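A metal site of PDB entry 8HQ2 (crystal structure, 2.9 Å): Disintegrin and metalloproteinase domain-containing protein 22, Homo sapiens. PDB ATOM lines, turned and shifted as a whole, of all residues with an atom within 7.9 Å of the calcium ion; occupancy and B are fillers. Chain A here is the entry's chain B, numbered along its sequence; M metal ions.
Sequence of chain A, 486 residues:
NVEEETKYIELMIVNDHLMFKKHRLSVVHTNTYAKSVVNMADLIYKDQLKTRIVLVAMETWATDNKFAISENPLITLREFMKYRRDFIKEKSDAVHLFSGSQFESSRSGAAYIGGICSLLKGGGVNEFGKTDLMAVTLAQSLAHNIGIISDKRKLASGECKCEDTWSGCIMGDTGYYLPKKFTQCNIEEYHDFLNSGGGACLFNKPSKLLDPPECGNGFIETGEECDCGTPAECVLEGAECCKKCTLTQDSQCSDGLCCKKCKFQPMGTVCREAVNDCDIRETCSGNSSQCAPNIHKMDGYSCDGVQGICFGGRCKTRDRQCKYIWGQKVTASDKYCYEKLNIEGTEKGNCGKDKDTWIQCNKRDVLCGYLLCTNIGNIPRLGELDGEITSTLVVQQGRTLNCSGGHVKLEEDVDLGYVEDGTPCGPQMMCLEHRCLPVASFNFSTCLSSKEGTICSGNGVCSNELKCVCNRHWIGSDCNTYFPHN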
ATOM      1  N   LYS A   7     -15.270  35.243  -5.748  1.00  0.00           N
ATOM      2  CA  LYS A   7     -15.842  34.035  -5.166  1.00  0.00           C
ATOM      3  C   LYS A   7     -17.159  33.709  -5.852  1.00  0.00           C
ATOM      4  O   LYS A   7     -17.946  34.608  -6.165  1.00  0.00           O
ATOM      5  CB  LYS A   7     -16.073  34.206  -3.651  1.00  0.00           C
ATOM      6  CG  LYS A   7     -14.804  34.160  -2.798  1.00  0.00           C
ATOM      7  CD  LYS A   7     -13.984  35.442  -2.899  1.00  0.00           C
ATOM      8  CE  LYS A   7     -14.766  36.660  -2.432  1.00  0.00           C
ATOM      9  NZ  LYS A   7     -13.922  37.894  -2.460  1.00  0.00           N
ATOM     10  N   TYR A   8     -17.394  32.427  -6.103  1.00  0.00           N
ATOM     11  CA  TYR A   8     -18.587  31.968  -6.805  1.00  0.00           C
ATOM     12  C   TYR A   8     -19.356  31.001  -5.911  1.00  0.00           C
ATOM     13  O   TYR A   8     -18.791  30.005  -5.440  1.00  0.00           O
ATOM     14  CB  TYR A   8     -18.226  31.296  -8.129  1.00  0.00           C
ATOM     15  CG  TYR A   8     -17.225  32.070  -8.966  1.00  0.00           C
ATOM     16  CD1 TYR A   8     -15.858  31.858  -8.813  1.00  0.00           C
ATOM     17  CD2 TYR A   8     -17.644  32.997  -9.899  1.00  0.00           C
ATOM     18  CE1 TYR A   8     -14.948  32.560  -9.570  1.00  0.00           C
ATOM     19  CE2 TYR A   8     -16.738  33.704 -10.663  1.00  0.00           C
ATOM     20  CZ  TYR A   8     -15.392  33.488 -10.503  1.00  0.00           C
ATOM     21  OH  TYR A   8     -14.494  34.198 -11.261  1.00  0.00           O
ATOM     22  N   ILE A   9     -20.637  31.285  -5.705  1.00  0.00           N
ATOM     23  CA  ILE A   9     -21.512  30.451  -4.894  1.00  0.00           C
ATOM     24  C   ILE A   9     -22.393  29.629  -5.836  1.00  0.00           C
ATOM     25  O   ILE A   9     -23.268  30.173  -6.512  1.00  0.00           O
ATOM     26  CB  ILE A   9     -22.371  31.290  -3.940  1.00  0.00           C
ATOM     27  CG1 ILE A   9     -21.496  32.023  -2.933  1.00  0.00           C
ATOM     28  CG2 ILE A   9     -23.402  30.411  -3.241  1.00  0.00           C
ATOM     29  CD1 ILE A   9     -22.276  32.887  -1.966  1.00  0.00           C
ATOM     30  N   GLU A  10     -22.162  28.320  -5.807  1.00  0.00           N
ATOM     31  CA  GLU A  10     -23.041  27.384  -6.551  1.00  0.00           C
ATOM     32  C   GLU A  10     -24.307  27.271  -5.700  1.00  0.00           C
ATOM     33  O   GLU A  10     -24.169  26.942  -4.500  1.00  0.00           O
ATOM     34  CB  GLU A  10     -22.358  26.026  -6.720  1.00  0.00           C
ATOM     35  CG  GLU A  10     -21.580  25.900  -8.015  1.00  0.00           C
ATOM     36  CD  GLU A  10     -20.344  25.023  -7.933  1.00  0.00           C
ATOM     37  OE1 GLU A  10     -19.903  24.731  -6.802  1.00  0.00           O
ATOM     38  OE2 GLU A  10     -19.833  24.624  -9.002  1.00  0.00           O
ATOM     39  N   LEU A  11     -25.469  27.511  -6.274  1.00  0.00           N
ATOM     40  CA  LEU A  11     -26.711  27.507  -5.509  1.00  0.00           C
ATOM     41  C   LEU A  11     -27.711  26.555  -6.150  1.00  0.00           C
ATOM     42  O   LEU A  11     -27.890  26.558  -7.373  1.00  0.00           O
ATOM     43  CB  LEU A  11     -27.303  28.917  -5.432  1.00  0.00           C
ATOM     44  CG  LEU A  11     -28.743  29.085  -4.934  1.00  0.00           C
ATOM     45  CD1 LEU A  11     -28.848  28.774  -3.458  1.00  0.00           C
ATOM     46  CD2 LEU A  11     -29.221  30.485  -5.228  1.00  0.00           C
ATOM     47  N   LYS A  91     -24.351  18.406  -6.487  1.00  0.00           N
ATOM     48  CA  LYS A  91     -23.217  19.157  -5.961  1.00  0.00           C
ATOM     49  C   LYS A  91     -23.549  20.647  -5.944  1.00  0.00           C
ATOM     50  O   LYS A  91     -23.882  21.228  -6.979  1.00  0.00           O
ATOM     51  CB  LYS A  91     -21.974  18.902  -6.808  1.00  0.00           C
ATOM     52  CG  LYS A  91     -21.436  17.487  -6.744  1.00  0.00           C
ATOM     53  CD  LYS A  91     -20.105  17.372  -7.474  1.00  0.00           C
ATOM     54  CE  LYS A  91     -19.516  15.973  -7.364  1.00  0.00           C
ATOM     55  NZ  LYS A  91     -18.194  15.889  -8.031  1.00  0.00           N
ATOM     56  N   SER A  92     -23.474  21.260  -4.765  1.00  0.00           N
ATOM     57  CA  SER A  92     -23.721  22.684  -4.652  1.00  0.00           C
ATOM     58  C   SER A  92     -23.027  23.209  -3.397  1.00  0.00           C
ATOM     59  O   SER A  92     -22.766  22.469  -2.448  1.00  0.00           O
ATOM     60  CB  SER A  92     -25.217  22.988  -4.580  1.00  0.00           C
ATOM     61  OG  SER A  92     -25.764  22.466  -3.389  1.00  0.00           O
ATOM     62  N   ASP A  93     -22.736  24.515  -3.417  1.00  0.00           N
ATOM     63  CA  ASP A  93     -22.221  25.168  -2.222  1.00  0.00           C
ATOM     64  C   ASP A  93     -23.327  25.385  -1.201  1.00  0.00           C
ATOM     65  O   ASP A  93     -23.069  25.343   0.009  1.00  0.00           O
ATOM     66  CB  ASP A  93     -21.576  26.505  -2.596  1.00  0.00           C
ATOM     67  CG  ASP A  93     -20.412  26.338  -3.540  1.00  0.00           C
ATOM     68  OD1 ASP A  93     -19.749  25.294  -3.481  1.00  0.00           O
ATOM     69  OD2 ASP A  93     -20.166  27.273  -4.338  1.00  0.00           O
ATOM     70  N   ALA A  94     -24.543  25.653  -1.665  1.00  0.00           N
ATOM     71  CA  ALA A  94     -25.666  25.925  -0.781  1.00  0.00           C
ATOM     72  C   ALA A  94     -26.960  25.441  -1.420  1.00  0.00           C
ATOM     73  O   ALA A  94     -27.135  25.536  -2.641  1.00  0.00           O
ATOM     74  CB  ALA A  94     -25.765  27.417  -0.435  1.00  0.00           C
ATOM     75  N   ILE A 116     -21.893  27.686   5.015  1.00  0.00           N
ATOM     76  CA  ILE A 116     -21.690  27.493   3.578  1.00  0.00           C
ATOM     77  C   ILE A 116     -20.806  26.277   3.329  1.00  0.00           C
ATOM     78  O   ILE A 116     -19.804  26.054   4.007  1.00  0.00           O
ATOM     79  CB  ILE A 116     -21.104  28.761   2.936  1.00  0.00           C
ATOM     80  CG1 ILE A 116     -20.964  28.593   1.418  1.00  0.00           C
ATOM     81  CG2 ILE A 116     -19.767  29.118   3.566  1.00  0.00           C
ATOM     82  CD1 ILE A 116     -22.280  28.370   0.706  1.00  0.00           C
ATOM     83  N   CYS A 117     -21.218  25.461   2.352  1.00  0.00           N
ATOM     84  CA  CYS A 117     -20.496  24.271   1.895  1.00  0.00           C
ATOM     85  C   CYS A 117     -20.371  23.207   2.973  1.00  0.00           C
ATOM     86  O   CYS A 117     -19.479  22.365   2.909  1.00  0.00           O
ATOM     87  CB  CYS A 117     -19.124  24.641   1.350  1.00  0.00           C
ATOM     88  SG  CYS A 117     -19.235  25.604  -0.129  1.00  0.00           S
ATOM     89  N   GLY A 199     -15.625  28.847   3.814  1.00  0.00           N
ATOM     90  CA  GLY A 199     -15.990  28.903   2.412  1.00  0.00           C
ATOM     91  C   GLY A 199     -14.858  28.684   1.427  1.00  0.00           C
ATOM     92  O   GLY A 199     -14.720  29.428   0.453  1.00  0.00           O
ATOM     93  N   ALA A 200     -14.047  27.646   1.657  1.00  0.00           N
ATOM     94  CA  ALA A 200     -12.956  27.336   0.727  1.00  0.00           C
ATOM     95  C   ALA A 200     -13.507  26.933  -0.629  1.00  0.00           C
ATOM     96  O   ALA A 200     -12.932  27.284  -1.671  1.00  0.00           O
ATOM     97  CB  ALA A 200     -12.084  26.219   1.312  1.00  0.00           C
ATOM     98  N   CYS A 201     -14.597  26.179  -0.643  1.00  0.00           N
ATOM     99  CA  CYS A 201     -15.291  25.801  -1.873  1.00  0.00           C
ATOM    100  C   CYS A 201     -15.581  26.991  -2.776  1.00  0.00           C
ATOM    101  O   CYS A 201     -15.555  26.861  -4.007  1.00  0.00           O
ATOM    102  CB  CYS A 201     -16.603  25.158  -1.499  1.00  0.00           C
ATOM    103  SG  CYS A 201     -17.358  26.256  -0.314  1.00  0.00           S
ATOM    104  N   LEU A 202     -15.893  28.152  -2.190  1.00  0.00           N
ATOM    105  CA  LEU A 202     -16.337  29.310  -2.956  1.00  0.00           C
ATOM    106  C   LEU A 202     -15.347  29.723  -4.045  1.00  0.00           C
ATOM    107  O   LEU A 202     -15.739  30.402  -4.991  1.00  0.00           O
ATOM    108  CB  LEU A 202     -16.574  30.494  -2.023  1.00  0.00           C
ATOM    109  CG  LEU A 202     -17.640  30.351  -0.948  1.00  0.00           C
ATOM    110  CD1 LEU A 202     -17.891  31.690  -0.283  1.00  0.00           C
ATOM    111  CD2 LEU A 202     -18.930  29.785  -1.525  1.00  0.00           C
ATOM    112  N   PHE A 203     -14.081  29.325  -3.917  1.00  0.00           N
ATOM    113  CA  PHE A 203     -13.057  29.711  -4.873  1.00  0.00           C
ATOM    114  C   PHE A 203     -13.032  28.828  -6.115  1.00  0.00           C
ATOM    115  O   PHE A 203     -12.362  29.177  -7.091  1.00  0.00           O
ATOM    116  CB  PHE A 203     -11.703  29.716  -4.172  1.00  0.00           C
ATOM    117  CG  PHE A 203     -11.670  30.628  -2.969  1.00  0.00           C
ATOM    118  CD1 PHE A 203     -12.074  30.165  -1.725  1.00  0.00           C
ATOM    119  CD2 PHE A 203     -11.298  31.950  -3.097  1.00  0.00           C
ATOM    120  CE1 PHE A 203     -12.059  31.002  -0.622  1.00  0.00           C
ATOM    121  CE2 PHE A 203     -11.279  32.789  -2.007  1.00  0.00           C
ATOM    122  CZ  PHE A 203     -11.663  32.316  -0.767  1.00  0.00           C
ATOM    123  N   ASN A 204     -13.716  27.689  -6.099  1.00  0.00           N
ATOM    124  CA  ASN A 204     -13.894  26.921  -7.320  1.00  0.00           C
ATOM    125  C   ASN A 204     -14.819  27.656  -8.276  1.00  0.00           C
ATOM    126  O   ASN A 204     -15.817  28.264  -7.865  1.00  0.00           O
ATOM    127  CB  ASN A 204     -14.445  25.528  -7.003  1.00  0.00           C
ATOM    128  CG  ASN A 204     -15.820  25.285  -7.594  1.00  0.00           C
ATOM    129  OD1 ASN A 204     -16.821  25.793  -7.089  1.00  0.00           O
ATOM    130  ND2 ASN A 204     -15.872  24.520  -8.673  1.00  0.00           N
ATOM    131  N   LYS A 205     -14.493  27.643  -9.565  1.00  0.00           N
ATOM    132  CA  LYS A 205     -15.292  28.305 -10.579  1.00  0.00           C
ATOM    133  C   LYS A 205     -16.234  27.305 -11.241  1.00  0.00           C
ATOM    134  O   LYS A 205     -15.792  26.205 -11.615  1.00  0.00           O
ATOM    135  CB  LYS A 205     -14.393  28.937 -11.642  1.00  0.00           C
ATOM    136  CG  LYS A 205     -15.062  29.980 -12.516  1.00  0.00           C
ATOM    137  CD  LYS A 205     -14.026  30.644 -13.400  1.00  0.00           C
ATOM    138  CE  LYS A 205     -14.613  31.770 -14.228  1.00  0.00           C
ATOM    139  NZ  LYS A 205     -13.615  32.354 -15.166  1.00  0.00           N
ATOM    140  N   PRO A 206     -17.521  27.624 -11.382  1.00  0.00           N
ATOM    141  CA  PRO A 206     -18.483  26.621 -11.857  1.00  0.00           C
ATOM    142  C   PRO A 206     -18.202  26.210 -13.301  1.00  0.00           C
ATOM    143  O   PRO A 206     -17.991  27.048 -14.178  1.00  0.00           O
ATOM    144  CB  PRO A 206     -19.834  27.329 -11.740  1.00  0.00           C
ATOM    145  CG  PRO A 206     -19.604  28.397 -10.721  1.00  0.00           C
ATOM    146  CD  PRO A 206     -18.196  28.849 -10.928  1.00  0.00           C
HETATM  147 CA    CA M   1     -17.983  25.903  -5.221  1.00  0.00          CA
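The calcium ion is bound by OD1 of Asn 204 (2.2 Å), OD1 of Asp 93 (2.6 Å), OD2 of Asp 93 (2.7 Å), OE1 of Glu 10 (2.7 Å) and O of Cys 201 (2.9 Å).
The calcium ion has five donor atoms within binding distance.
N of Cys 117 is in hydrogen-bond range of O of Asp 93.
The backbone NH of Ala 94 lies within hydrogen-bond range of the backbone carbonyl oxygen of Glu 10 (3.1 Å).
The side-chain sulfur (SG) of Cys 201 forms a disulfide with the side-chain sulfur (SG) of Cys 117, 2.0 Å away.
Four residues have an atom within 4 Å of the calcium ion: Glu 10, Asp 93, Cys 201 and Asn 204.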
